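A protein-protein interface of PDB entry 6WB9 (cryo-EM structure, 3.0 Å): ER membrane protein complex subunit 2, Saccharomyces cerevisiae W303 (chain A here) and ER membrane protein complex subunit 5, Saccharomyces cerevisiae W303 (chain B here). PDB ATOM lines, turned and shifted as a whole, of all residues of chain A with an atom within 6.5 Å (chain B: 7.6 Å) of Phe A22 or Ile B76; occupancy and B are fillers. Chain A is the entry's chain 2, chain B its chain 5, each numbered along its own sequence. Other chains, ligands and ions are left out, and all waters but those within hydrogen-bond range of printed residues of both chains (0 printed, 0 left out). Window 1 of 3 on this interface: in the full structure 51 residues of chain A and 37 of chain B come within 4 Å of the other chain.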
ATOM      1  N   GLU A   8      30.929 -12.128  -3.346  1.00  0.00           N
ATOM      2  CA  GLU A   8      30.728 -13.564  -3.513  1.00  0.00           C
ATOM      3  C   GLU A   8      29.298 -13.893  -3.920  1.00  0.00           C
ATOM      4  O   GLU A   8      29.083 -14.845  -4.679  1.00  0.00           O
ATOM      5  CB  GLU A   8      31.106 -14.305  -2.234  1.00  0.00           C
ATOM      6  CG  GLU A   8      32.584 -14.220  -1.885  1.00  0.00           C
ATOM      7  CD  GLU A   8      33.486 -14.760  -2.980  1.00  0.00           C
ATOM      8  OE1 GLU A   8      33.173 -15.827  -3.551  1.00  0.00           O
ATOM      9  OE2 GLU A   8      34.513 -14.116  -3.272  1.00  0.00           O
ATOM     10  N   LYS A   9      28.321 -13.096  -3.475  1.00  0.00           N
ATOM     11  CA  LYS A   9      26.945 -13.269  -3.933  1.00  0.00           C
ATOM     12  C   LYS A   9      26.811 -12.979  -5.422  1.00  0.00           C
ATOM     13  O   LYS A   9      26.186 -13.753  -6.155  1.00  0.00           O
ATOM     14  CB  LYS A   9      26.013 -12.368  -3.126  1.00  0.00           C
ATOM     15  CG  LYS A   9      24.573 -12.365  -3.594  1.00  0.00           C
ATOM     16  CD  LYS A   9      23.720 -11.489  -2.699  1.00  0.00           C
ATOM     17  CE  LYS A   9      22.297 -11.393  -3.206  1.00  0.00           C
ATOM     18  NZ  LYS A   9      22.229 -10.710  -4.524  1.00  0.00           N
ATOM     19  N   THR A  12      28.463 -15.759  -7.397  1.00  0.00           N
ATOM     20  CA  THR A  12      27.649 -16.968  -7.486  1.00  0.00           C
ATOM     21  C   THR A  12      26.444 -16.778  -8.394  1.00  0.00           C
ATOM     22  O   THR A  12      26.010 -17.738  -9.034  1.00  0.00           O
ATOM     23  CB  THR A  12      27.178 -17.420  -6.104  1.00  0.00           C
ATOM     24  OG1 THR A  12      26.624 -16.308  -5.396  1.00  0.00           O
ATOM     25  CG2 THR A  12      28.329 -18.008  -5.312  1.00  0.00           C
ATOM     26  N   ILE A  13      25.884 -15.569  -8.463  1.00  0.00           N
ATOM     27  CA  ILE A  13      24.813 -15.334  -9.428  1.00  0.00           C
ATOM     28  C   ILE A  13      25.377 -15.295 -10.848  1.00  0.00           C
ATOM     29  O   ILE A  13      24.713 -15.718 -11.800  1.00  0.00           O
ATOM     30  CB  ILE A  13      24.033 -14.055  -9.055  1.00  0.00           C
ATOM     31  CG1 ILE A  13      23.384 -14.225  -7.688  1.00  0.00           C
ATOM     32  CG2 ILE A  13      22.906 -13.774 -10.023  1.00  0.00           C
ATOM     33  CD1 ILE A  13      22.778 -12.968  -7.144  1.00  0.00           C
ATOM     34  N   THR A  16      26.671 -19.362 -11.638  1.00  0.00           N
ATOM     35  CA  THR A  16      25.547 -20.276 -11.754  1.00  0.00           C
ATOM     36  C   THR A  16      24.427 -19.729 -12.624  1.00  0.00           C
ATOM     37  O   THR A  16      23.450 -20.448 -12.839  1.00  0.00           O
ATOM     38  CB  THR A  16      24.999 -20.619 -10.371  1.00  0.00           C
ATOM     39  OG1 THR A  16      24.313 -19.486  -9.828  1.00  0.00           O
ATOM     40  CG2 THR A  16      26.136 -21.005  -9.444  1.00  0.00           C
ATOM     41  N   ALA A  18      22.072 -17.425 -12.184  1.00  0.00           N
ATOM     42  CA  ALA A  18      20.776 -17.381 -11.523  1.00  0.00           C
ATOM     43  C   ALA A  18      19.918 -16.222 -12.005  1.00  0.00           C
ATOM     44  O   ALA A  18      18.692 -16.284 -11.869  1.00  0.00           O
ATOM     45  CB  ALA A  18      20.962 -17.296 -10.011  1.00  0.00           C
ATOM     46  N   TYR A  19      20.528 -15.186 -12.595  1.00  0.00           N
ATOM     47  CA  TYR A  19      19.782 -14.043 -13.117  1.00  0.00           C
ATOM     48  C   TYR A  19      18.899 -14.412 -14.303  1.00  0.00           C
ATOM     49  O   TYR A  19      17.991 -13.646 -14.643  1.00  0.00           O
ATOM     50  CB  TYR A  19      20.738 -12.914 -13.514  1.00  0.00           C
ATOM     51  CG  TYR A  19      21.775 -13.271 -14.561  1.00  0.00           C
ATOM     52  CD1 TYR A  19      23.003 -13.807 -14.195  1.00  0.00           C
ATOM     53  CD2 TYR A  19      21.541 -13.038 -15.910  1.00  0.00           C
ATOM     54  CE1 TYR A  19      23.953 -14.125 -15.143  1.00  0.00           C
ATOM     55  CE2 TYR A  19      22.484 -13.357 -16.864  1.00  0.00           C
ATOM     56  CZ  TYR A  19      23.688 -13.897 -16.473  1.00  0.00           C
ATOM     57  OH  TYR A  19      24.635 -14.211 -17.417  1.00  0.00           O
ATOM     58  N   THR A  20      19.170 -15.548 -14.949  1.00  0.00           N
ATOM     59  CA  THR A  20      18.260 -16.105 -15.939  1.00  0.00           C
ATOM     60  C   THR A  20      16.895 -16.417 -15.336  1.00  0.00           C
ATOM     61  O   THR A  20      15.862 -16.192 -15.981  1.00  0.00           O
ATOM     62  CB  THR A  20      18.894 -17.363 -16.537  1.00  0.00           C
ATOM     63  OG1 THR A  20      20.169 -17.031 -17.095  1.00  0.00           O
ATOM     64  CG2 THR A  20      18.025 -17.965 -17.620  1.00  0.00           C
ATOM     65  N   GLN A  21      16.861 -16.880 -14.085  1.00  0.00           N
ATOM     66  CA  GLN A  21      15.625 -17.319 -13.451  1.00  0.00           C
ATOM     67  C   GLN A  21      15.085 -16.305 -12.447  1.00  0.00           C
ATOM     68  O   GLN A  21      14.283 -16.666 -11.582  1.00  0.00           O
ATOM     69  CB  GLN A  21      15.844 -18.667 -12.769  1.00  0.00           C
ATOM     70  CG  GLN A  21      16.423 -19.718 -13.686  1.00  0.00           C
ATOM     71  CD  GLN A  21      15.363 -20.502 -14.428  1.00  0.00           C
ATOM     72  OE1 GLN A  21      15.478 -20.741 -15.630  1.00  0.00           O
ATOM     73  NE2 GLN A  21      14.328 -20.920 -13.711  1.00  0.00           N
ATOM     74  N   PHE A  22      15.499 -15.047 -12.547  1.00  0.00           N
ATOM     75  CA  PHE A  22      15.136 -14.052 -11.551  1.00  0.00           C
ATOM     76  C   PHE A  22      13.837 -13.345 -11.911  1.00  0.00           C
ATOM     77  O   PHE A  22      13.490 -13.187 -13.085  1.00  0.00           O
ATOM     78  CB  PHE A  22      16.254 -13.022 -11.385  1.00  0.00           C
ATOM     79  CG  PHE A  22      17.260 -13.375 -10.325  1.00  0.00           C
ATOM     80  CD1 PHE A  22      17.167 -14.562  -9.619  1.00  0.00           C
ATOM     81  CD2 PHE A  22      18.290 -12.504 -10.024  1.00  0.00           C
ATOM     82  CE1 PHE A  22      18.091 -14.877  -8.643  1.00  0.00           C
ATOM     83  CE2 PHE A  22      19.214 -12.812  -9.050  1.00  0.00           C
ATOM     84  CZ  PHE A  22      19.114 -14.000  -8.360  1.00  0.00           C
ATOM     85  N   ASN A  23      13.119 -12.916 -10.875  1.00  0.00           N
ATOM     86  CA  ASN A  23      11.933 -12.095 -11.038  1.00  0.00           C
ATOM     87  C   ASN A  23      12.334 -10.688 -11.476  1.00  0.00           C
ATOM     88  O   ASN A  23      13.495 -10.299 -11.335  1.00  0.00           O
ATOM     89  CB  ASN A  23      11.153 -12.039  -9.724  1.00  0.00           C
ATOM     90  CG  ASN A  23      10.723 -13.405  -9.244  1.00  0.00           C
ATOM     91  OD1 ASN A  23      10.908 -13.751  -8.078  1.00  0.00           O
ATOM     92  ND2 ASN A  23      10.148 -14.195 -10.142  1.00  0.00           N
ATOM     93  N   PRO A  24      11.396  -9.913 -12.041  1.00  0.00           N
ATOM     94  CA  PRO A  24      11.695  -8.496 -12.315  1.00  0.00           C
ATOM     95  C   PRO A  24      12.005  -7.679 -11.073  1.00  0.00           C
ATOM     96  O   PRO A  24      12.817  -6.748 -11.149  1.00  0.00           O
ATOM     97  CB  PRO A  24      10.419  -8.004 -13.005  1.00  0.00           C
ATOM     98  CG  PRO A  24       9.881  -9.203 -13.662  1.00  0.00           C
ATOM     99  CD  PRO A  24      10.177 -10.350 -12.747  1.00  0.00           C
ATOM    100  N   GLU A  25      11.393  -8.000  -9.930  1.00  0.00           N
ATOM    101  CA  GLU A  25      11.789  -7.361  -8.679  1.00  0.00           C
ATOM    102  C   GLU A  25      13.183  -7.804  -8.260  1.00  0.00           C
ATOM    103  O   GLU A  25      13.996  -6.986  -7.809  1.00  0.00           O
ATOM    104  CB  GLU A  25      10.773  -7.682  -7.584  1.00  0.00           C
ATOM    105  CG  GLU A  25      11.042  -6.987  -6.261  1.00  0.00           C
ATOM    106  CD  GLU A  25      10.244  -7.586  -5.119  1.00  0.00           C
ATOM    107  OE1 GLU A  25       9.618  -8.646  -5.323  1.00  0.00           O
ATOM    108  OE2 GLU A  25      10.247  -6.999  -4.017  1.00  0.00           O
ATOM    109  N   GLN A  26      13.480  -9.096  -8.422  1.00  0.00           N
ATOM    110  CA  GLN A  26      14.815  -9.598  -8.129  1.00  0.00           C
ATOM    111  C   GLN A  26      15.838  -9.080  -9.127  1.00  0.00           C
ATOM    112  O   GLN A  26      16.982  -8.819  -8.748  1.00  0.00           O
ATOM    113  CB  GLN A  26      14.808 -11.125  -8.107  1.00  0.00           C
ATOM    114  CG  GLN A  26      13.968 -11.714  -6.990  1.00  0.00           C
ATOM    115  CD  GLN A  26      13.910 -13.225  -7.035  1.00  0.00           C
ATOM    116  OE1 GLN A  26      14.512 -13.855  -7.901  1.00  0.00           O
ATOM    117  NE2 GLN A  26      13.177 -13.815  -6.101  1.00  0.00           N
ATOM    118  N   LEU A  27      15.443  -8.882 -10.388  1.00  0.00           N
ATOM    119  CA  LEU A  27      16.352  -8.274 -11.355  1.00  0.00           C
ATOM    120  C   LEU A  27      16.586  -6.799 -11.057  1.00  0.00           C
ATOM    121  O   LEU A  27      17.691  -6.297 -11.284  1.00  0.00           O
ATOM    122  CB  LEU A  27      15.813  -8.442 -12.775  1.00  0.00           C
ATOM    123  CG  LEU A  27      16.054  -9.780 -13.467  1.00  0.00           C
ATOM    124  CD1 LEU A  27      15.329  -9.814 -14.794  1.00  0.00           C
ATOM    125  CD2 LEU A  27      17.534 -10.013 -13.665  1.00  0.00           C
ATOM    126  N   LEU A  30      18.901  -6.789  -8.154  1.00  0.00           N
ATOM    127  CA  LEU A  30      20.198  -7.244  -8.632  1.00  0.00           C
ATOM    128  C   LEU A  30      20.929  -6.149  -9.394  1.00  0.00           C
ATOM    129  O   LEU A  30      22.137  -5.978  -9.220  1.00  0.00           O
ATOM    130  CB  LEU A  30      20.018  -8.472  -9.517  1.00  0.00           C
ATOM    131  CG  LEU A  30      21.313  -9.141  -9.956  1.00  0.00           C
ATOM    132  CD1 LEU A  30      22.038  -9.652  -8.737  1.00  0.00           C
ATOM    133  CD2 LEU A  30      21.002 -10.260 -10.908  1.00  0.00           C
ATOM    134  N   MET A  56      27.228  -9.986 -16.941  1.00  0.00           N
ATOM    135  CA  MET A  56      25.999 -10.257 -16.198  1.00  0.00           C
ATOM    136  C   MET A  56      25.161  -8.992 -16.022  1.00  0.00           C
ATOM    137  O   MET A  56      23.929  -9.036 -16.124  1.00  0.00           O
ATOM    138  CB  MET A  56      26.360 -10.875 -14.848  1.00  0.00           C
ATOM    139  CG  MET A  56      25.270 -10.880 -13.808  1.00  0.00           C
ATOM    140  SD  MET A  56      25.955 -11.310 -12.208  1.00  0.00           S
ATOM    141  CE  MET A  56      24.684 -10.688 -11.134  1.00  0.00           C
ATOM    142  N   VAL A  60      21.358  -8.272 -17.318  1.00  0.00           N
ATOM    143  CA  VAL A  60      20.322  -7.768 -16.419  1.00  0.00           C
ATOM    144  C   VAL A  60      19.708  -6.484 -16.972  1.00  0.00           C
ATOM    145  O   VAL A  60      18.486  -6.297 -16.932  1.00  0.00           O
ATOM    146  CB  VAL A  60      20.902  -7.581 -15.004  1.00  0.00           C
ATOM    147  CG1 VAL A  60      19.957  -6.803 -14.114  1.00  0.00           C
ATOM    148  CG2 VAL A  60      21.169  -8.928 -14.382  1.00  0.00           C
ATOM    149  N   TYR B  73      27.904 -16.020   4.079  1.00  0.00           N
ATOM    150  CA  TYR B  73      27.381 -15.949   2.728  1.00  0.00           C
ATOM    151  C   TYR B  73      26.092 -15.148   2.727  1.00  0.00           C
ATOM    152  O   TYR B  73      25.315 -15.206   3.683  1.00  0.00           O
ATOM    153  CB  TYR B  73      27.112 -17.346   2.154  1.00  0.00           C
ATOM    154  CG  TYR B  73      28.263 -18.316   2.272  1.00  0.00           C
ATOM    155  CD1 TYR B  73      29.294 -18.313   1.344  1.00  0.00           C
ATOM    156  CD2 TYR B  73      28.315 -19.237   3.309  1.00  0.00           C
ATOM    157  CE1 TYR B  73      30.348 -19.196   1.448  1.00  0.00           C
ATOM    158  CE2 TYR B  73      29.365 -20.125   3.421  1.00  0.00           C
ATOM    159  CZ  TYR B  73      30.377 -20.098   2.489  1.00  0.00           C
ATOM    160  OH  TYR B  73      31.421 -20.982   2.590  1.00  0.00           O
ATOM    161  N   LEU B  74      25.877 -14.390   1.662  1.00  0.00           N
ATOM    162  CA  LEU B  74      24.543 -13.823   1.542  1.00  0.00           C
ATOM    163  C   LEU B  74      23.645 -14.782   0.768  1.00  0.00           C
ATOM    164  O   LEU B  74      24.109 -15.444  -0.162  1.00  0.00           O
ATOM    165  CB  LEU B  74      24.584 -12.479   0.825  1.00  0.00           C
ATOM    166  CG  LEU B  74      25.220 -11.301   1.554  1.00  0.00           C
ATOM    167  CD1 LEU B  74      25.187 -10.072   0.674  1.00  0.00           C
ATOM    168  CD2 LEU B  74      24.499 -11.038   2.853  1.00  0.00           C
ATOM    169  N   PRO B  75      22.373 -14.894   1.143  1.00  0.00           N
ATOM    170  CA  PRO B  75      21.438 -15.682   0.334  1.00  0.00           C
ATOM    171  C   PRO B  75      21.185 -15.012  -1.005  1.00  0.00           C
ATOM    172  O   PRO B  75      21.145 -13.784  -1.108  1.00  0.00           O
ATOM    173  CB  PRO B  75      20.170 -15.722   1.191  1.00  0.00           C
ATOM    174  CG  PRO B  75      20.283 -14.545   2.084  1.00  0.00           C
ATOM    175  CD  PRO B  75      21.741 -14.385   2.369  1.00  0.00           C
ATOM    176  N   ILE B  76      21.024 -15.834  -2.038  1.00  0.00           N
ATOM    177  CA  ILE B  76      20.939 -15.314  -3.397  1.00  0.00           C
ATOM    178  C   ILE B  76      19.561 -14.721  -3.668  1.00  0.00           C
ATOM    179  O   ILE B  76      19.444 -13.608  -4.193  1.00  0.00           O
ATOM    180  CB  ILE B  76      21.310 -16.422  -4.403  1.00  0.00           C
ATOM    181  CG1 ILE B  76      22.831 -16.604  -4.405  1.00  0.00           C
ATOM    182  CG2 ILE B  76      20.756 -16.127  -5.795  1.00  0.00           C
ATOM    183  CD1 ILE B  76      23.383 -17.345  -5.588  1.00  0.00           C
ATOM    184  N   GLU B  77      18.501 -15.432  -3.284  1.00  0.00           N
ATOM    185  CA  GLU B  77      17.154 -14.963  -3.590  1.00  0.00           C
ATOM    186  C   GLU B  77      16.728 -13.825  -2.667  1.00  0.00           C
ATOM    187  O   GLU B  77      16.423 -12.722  -3.129  1.00  0.00           O
ATOM    188  CB  GLU B  77      16.157 -16.120  -3.507  1.00  0.00           C
ATOM    189  CG  GLU B  77      14.715 -15.678  -3.681  1.00  0.00           C
ATOM    190  CD  GLU B  77      13.779 -16.820  -4.018  1.00  0.00           C
ATOM    191  OE1 GLU B  77      14.207 -17.990  -3.936  1.00  0.00           O
ATOM    192  OE2 GLU B  77      12.614 -16.544  -4.370  1.00  0.00           O
ATOM    193  N   SER B  78      16.703 -14.078  -1.362  1.00  0.00           N
ATOM    194  CA  SER B  78      16.181 -13.101  -0.418  1.00  0.00           C
ATOM    195  C   SER B  78      17.178 -11.968  -0.197  1.00  0.00           C
ATOM    196  O   SER B  78      18.396 -12.161  -0.252  1.00  0.00           O
ATOM    197  CB  SER B  78      15.844 -13.767   0.917  1.00  0.00           C
ATOM    198  OG  SER B  78      16.982 -14.386   1.486  1.00  0.00           O
ATOM    199  N   ASN B  79      16.641 -10.774   0.048  1.00  0.00           N
ATOM    200  CA  ASN B  79      17.435  -9.561   0.242  1.00  0.00           C
ATOM    201  C   ASN B  79      16.960  -8.890   1.527  1.00  0.00           C
ATOM    202  O   ASN B  79      16.072  -8.035   1.505  1.00  0.00           O
ATOM    203  CB  ASN B  79      17.316  -8.631  -0.959  1.00  0.00           C
ATOM    204  CG  ASN B  79      17.751  -9.292  -2.249  1.00  0.00           C
ATOM    205  OD1 ASN B  79      16.953  -9.469  -3.169  1.00  0.00           O
ATOM    206  ND2 ASN B  79      19.024  -9.662  -2.325  1.00  0.00           N
ATOM    207  N   LYS B  82      19.790 -10.966   6.747  1.00  0.00           N
ATOM    208  CA  LYS B  82      20.109 -12.330   7.144  1.00  0.00           C
ATOM    209  C   LYS B  82      21.357 -12.787   6.404  1.00  0.00           C
ATOM    210  O   LYS B  82      21.436 -12.663   5.177  1.00  0.00           O
ATOM    211  CB  LYS B  82      18.946 -13.281   6.853  1.00  0.00           C
ATOM    212  CG  LYS B  82      19.181 -14.701   7.338  1.00  0.00           C
ATOM    213  CD  LYS B  82      18.038 -15.620   6.947  1.00  0.00           C
ATOM    214  CE  LYS B  82      17.924 -15.743   5.438  1.00  0.00           C
ATOM    215  NZ  LYS B  82      19.163 -16.304   4.835  1.00  0.00           N
ATOM    216  N   ILE B  84      24.050 -16.132   6.129  1.00  0.00           N
ATOM    217  CA  ILE B  84      24.131 -17.563   6.393  1.00  0.00           C
ATOM    218  C   ILE B  84      25.567 -17.920   6.746  1.00  0.00           C
ATOM    219  O   ILE B  84      26.488 -17.654   5.968  1.00  0.00           O
ATOM    220  CB  ILE B  84      23.643 -18.365   5.178  1.00  0.00           C
ATOM    221  CG1 ILE B  84      22.154 -18.118   4.967  1.00  0.00           C
ATOM    222  CG2 ILE B  84      23.925 -19.840   5.355  1.00  0.00           C
ATOM    223  CD1 ILE B  84      21.733 -18.199   3.541  1.00  0.00           C
ATOM    224  N   ASP B 102      25.711 -24.254  -1.047  1.00  0.00           N
ATOM    225  CA  ASP B 102      24.879 -23.970  -2.208  1.00  0.00           C
ATOM    226  C   ASP B 102      23.401 -24.192  -1.918  1.00  0.00           C
ATOM    227  O   ASP B 102      22.550 -23.536  -2.524  1.00  0.00           O
ATOM    228  CB  ASP B 102      25.336 -24.833  -3.378  1.00  0.00           C
ATOM    229  CG  ASP B 102      26.829 -24.738  -3.610  1.00  0.00           C
ATOM    230  OD1 ASP B 102      27.336 -23.607  -3.762  1.00  0.00           O
ATOM    231  OD2 ASP B 102      27.502 -25.789  -3.622  1.00  0.00           O
ATOM    232  N   LEU B 104      22.049 -23.830   1.262  1.00  0.00           N
ATOM    233  CA  LEU B 104      21.622 -22.882   2.285  1.00  0.00           C
ATOM    234  C   LEU B 104      21.312 -21.515   1.690  1.00  0.00           C
ATOM    235  O   LEU B 104      20.362 -20.852   2.119  1.00  0.00           O
ATOM    236  CB  LEU B 104      22.698 -22.751   3.364  1.00  0.00           C
ATOM    237  CG  LEU B 104      22.764 -23.740   4.531  1.00  0.00           C
ATOM    238  CD1 LEU B 104      24.147 -23.721   5.143  1.00  0.00           C
ATOM    239  CD2 LEU B 104      21.756 -23.401   5.579  1.00  0.00           C
ATOM    240  N   ILE B 105      22.097 -21.077   0.700  1.00  0.00           N
ATOM    241  CA  ILE B 105      21.915 -19.753   0.115  1.00  0.00           C
ATOM    242  C   ILE B 105      20.977 -19.757  -1.080  1.00  0.00           C
ATOM    243  O   ILE B 105      20.566 -18.680  -1.535  1.00  0.00           O
ATOM    244  CB  ILE B 105      23.270 -19.143  -0.294  1.00  0.00           C
ATOM    245  CG1 ILE B 105      23.816 -19.822  -1.550  1.00  0.00           C
ATOM    246  CG2 ILE B 105      24.252 -19.273   0.840  1.00  0.00           C
ATOM    247  CD1 ILE B 105      25.178 -19.333  -1.972  1.00  0.00           C
ATOM    248  N   GLY B 106      20.622 -20.924  -1.602  1.00  0.00           N
ATOM    249  CA  GLY B 106      19.677 -20.993  -2.693  1.00  0.00           C
ATOM    250  C   GLY B 106      20.285 -20.987  -4.074  1.00  0.00           C
ATOM    251  O   GLY B 106      19.639 -20.520  -5.018  1.00  0.00           O
ATOM    252  N   SER B 107      21.501 -21.487  -4.228  1.00  0.00           N
ATOM    253  CA  SER B 107      22.141 -21.569  -5.530  1.00  0.00           C
ATOM    254  C   SER B 107      22.150 -23.013  -6.015  1.00  0.00           C
ATOM    255  O   SER B 107      21.739 -23.940  -5.313  1.00  0.00           O
ATOM    256  CB  SER B 107      23.561 -21.005  -5.480  1.00  0.00           C
ATOM    257  OG  SER B 107      24.404 -21.789  -4.663  1.00  0.00           O
ATOM    258  N   ASN B 108      22.619 -23.190  -7.239  1.00  0.00           N
ATOM    259  CA  ASN B 108      22.784 -24.499  -7.847  1.00  0.00           C
ATOM    260  C   ASN B 108      24.121 -24.496  -8.571  1.00  0.00           C
ATOM    261  O   ASN B 108      24.283 -23.738  -9.533  1.00  0.00           O
ATOM    262  CB  ASN B 108      21.635 -24.795  -8.808  1.00  0.00           C
ATOM    263  CG  ASN B 108      21.379 -26.279  -8.977  1.00  0.00           C
ATOM    264  OD1 ASN B 108      22.282 -27.102  -8.843  1.00  0.00           O
ATOM    265  ND2 ASN B 108      20.134 -26.625  -9.276  1.00  0.00           N
ATOM    266  N   PHE B 115      19.632 -24.102 -15.322  1.00  0.00           N
ATOM    267  CA  PHE B 115      18.758 -22.953 -15.522  1.00  0.00           C
ATOM    268  C   PHE B 115      18.538 -22.606 -16.986  1.00  0.00           C
ATOM    269  O   PHE B 115      17.717 -21.727 -17.270  1.00  0.00           O
ATOM    270  CB  PHE B 115      19.323 -21.728 -14.802  1.00  0.00           C
ATOM    271  CG  PHE B 115      19.358 -21.863 -13.310  1.00  0.00           C
ATOM    272  CD1 PHE B 115      18.354 -22.529 -12.632  1.00  0.00           C
ATOM    273  CD2 PHE B 115      20.402 -21.320 -12.586  1.00  0.00           C
ATOM    274  CE1 PHE B 115      18.390 -22.648 -11.261  1.00  0.00           C
ATOM    275  CE2 PHE B 115      20.446 -21.436 -11.217  1.00  0.00           C
ATOM    276  CZ  PHE B 115      19.440 -22.100 -10.553  1.00  0.00           C
ATOM    277  N   LYS B 125      11.505 -12.236 -21.325  1.00  0.00           N
ATOM    278  CA  LYS B 125      12.006 -11.586 -20.116  1.00  0.00           C
ATOM    279  C   LYS B 125      11.734 -10.087 -20.143  1.00  0.00           C
ATOM    280  O   LYS B 125      11.335  -9.504 -19.125  1.00  0.00           O
ATOM    281  CB  LYS B 125      13.504 -11.847 -19.958  1.00  0.00           C
ATOM    282  CG  LYS B 125      13.893 -13.313 -19.918  1.00  0.00           C
ATOM    283  CD  LYS B 125      13.701 -13.912 -18.541  1.00  0.00           C
ATOM    284  CE  LYS B 125      14.718 -13.365 -17.561  1.00  0.00           C
ATOM    285  NZ  LYS B 125      14.588 -14.006 -16.228  1.00  0.00           N
ATOM    286  N   ILE B 128       7.961  -9.611 -19.507  1.00  0.00           N
ATOM    287  CA  ILE B 128       7.596  -9.802 -18.105  1.00  0.00           C
ATOM    288  C   ILE B 128       8.076  -8.627 -17.256  1.00  0.00           C
ATOM    289  O   ILE B 128       7.339  -8.128 -16.394  1.00  0.00           O
ATOM    290  CB  ILE B 128       8.141 -11.152 -17.600  1.00  0.00           C
ATOM    291  CG1 ILE B 128       7.390 -12.305 -18.263  1.00  0.00           C
ATOM    292  CG2 ILE B 128       8.000 -11.285 -16.095  1.00  0.00           C
ATOM    293  CD1 ILE B 128       7.934 -13.671 -17.912  1.00  0.00           C
ATOM    294  N   CYS B 129       9.283  -8.117 -17.532  1.00  0.00           N
ATOM    295  CA  CYS B 129       9.786  -6.974 -16.773  1.00  0.00           C
ATOM    296  C   CYS B 129       9.035  -5.691 -17.115  1.00  0.00           C
ATOM    297  O   CYS B 129       8.792  -4.859 -16.234  1.00  0.00           O
ATOM    298  CB  CYS B 129      11.284  -6.803 -17.015  1.00  0.00           C
ATOM    299  SG  CYS B 129      12.306  -8.073 -16.236  1.00  0.00           S
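The backbone carbonyl oxygen of Thr A20 is in hydrogen-bond range of the side-chain amino group of Lys B125, at 2.5 Å.
The backbone carbonyl oxygen (O) of Phe B115 sits close to the side-chain amide oxygen (OE1) of Gln A21 (2.9 Å).
The backbone carbonyl oxygen (O) of Phe A22 lies within hydrogen-bond range of the side-chain amino group (NZ) of Lys B125 (3.4 Å).
The side-chain carboxylate (OE2) of Glu B77 lies within hydrogen-bond range of the side-chain amide nitrogen (NE2) of Gln A26.
The backbone carbonyl oxygen (O) of Lys B125 lies within hydrogen-bond range of the side-chain sulfur (SG) of Cys B129 (3.4 Å).
N of Ile B76 is in hydrogen-bond range of O of Ile B105, at 2.9 Å.
The side-chain hydroxyl (OG1) of Thr A16 lies within hydrogen-bond range of the backbone carbonyl oxygen (O) of Thr A12, 2.6 Å away.
The backbone carbonyl oxygen (O) of Glu A8 is in hydrogen-bond range of the side-chain hydroxyl (OG1) of Thr A12 (2.9 Å).
The side-chain amide oxygen (OD1) of Asn A23 sits at hydrogen-bond distance from the side-chain amide nitrogen (NE2) of Gln A26, at 3.0 Å.
O of Ile A13 lies within hydrogen-bond range of N of Ala A18, at 3.2 Å.
Among the printed residues, pairs that only touch across the chains: Thr A16 with Phe B115, Thr A16 with Asn B108, Lys A9 with Pro B75, Thr A12 with Ile B76, Pro A24 with Cys B129, Pro A24 with Ile B128, Phe A22 with Ile B76, Lys A9 with Ile B76, Ile A13 with Ile B76, Lys A9 with Leu B74, Tyr A19 with Lys B125, Leu A27 with Cys B129, Thr A20 with Phe B115 and Lys A9 with Asn B79.
Of chain B, only Ile B76 and Lys B125 come within 4 Å of Phe A22.
Ile B76 touches four residues of chain A.
Of the printed residues of chain A, Glu B77 touches Gln A26.
Of the printed residues of chain B, Leu A27 touches Cys B129 (3.8 Å).
Printed residues of chain A within 4 Å of Phe B115: Thr A16 (3.2 Å), Thr A20 (3.8 Å) and Gln A21 (2.9 Å).
Printed residues of chain A within 4 Å of Asn B79: Lys A9.
Tyr B73 touches none of the printed residues of chain A.
The nearest residue of chain B that does not touch Phe A22 is Glu B77 (5.1 Å).
The nearest residue of chain A that does not touch Ile B76 is Ala A18 (4.4 Å).
The nearest printed residue of chain A that does not touch Lys B125 is Gln A21 (4.2 Å).
Hydrophobic or aromatic side chains of chain A that line the printed part of chain B: Ile A13, Phe A22, Pro A24 and Leu A27.
Along chain A the printed residues that touch a printed residue of chain B span positions 9 to 27.
Of the 19 printed residues of chain B, 10 touch a printed residue of chain A.
Printed residues of chain B that touch a printed residue of chain A: Leu B74, Pro B75, Ile B76, Glu B77, Asn B79, Asn B108, Phe B115, Lys B125, Ile B128 and Cys B129.
Along chain B the printed residues that touch a printed residue of chain A span positions 74 to 129.
Among the printed residues, 18 pairs touch across the chains.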
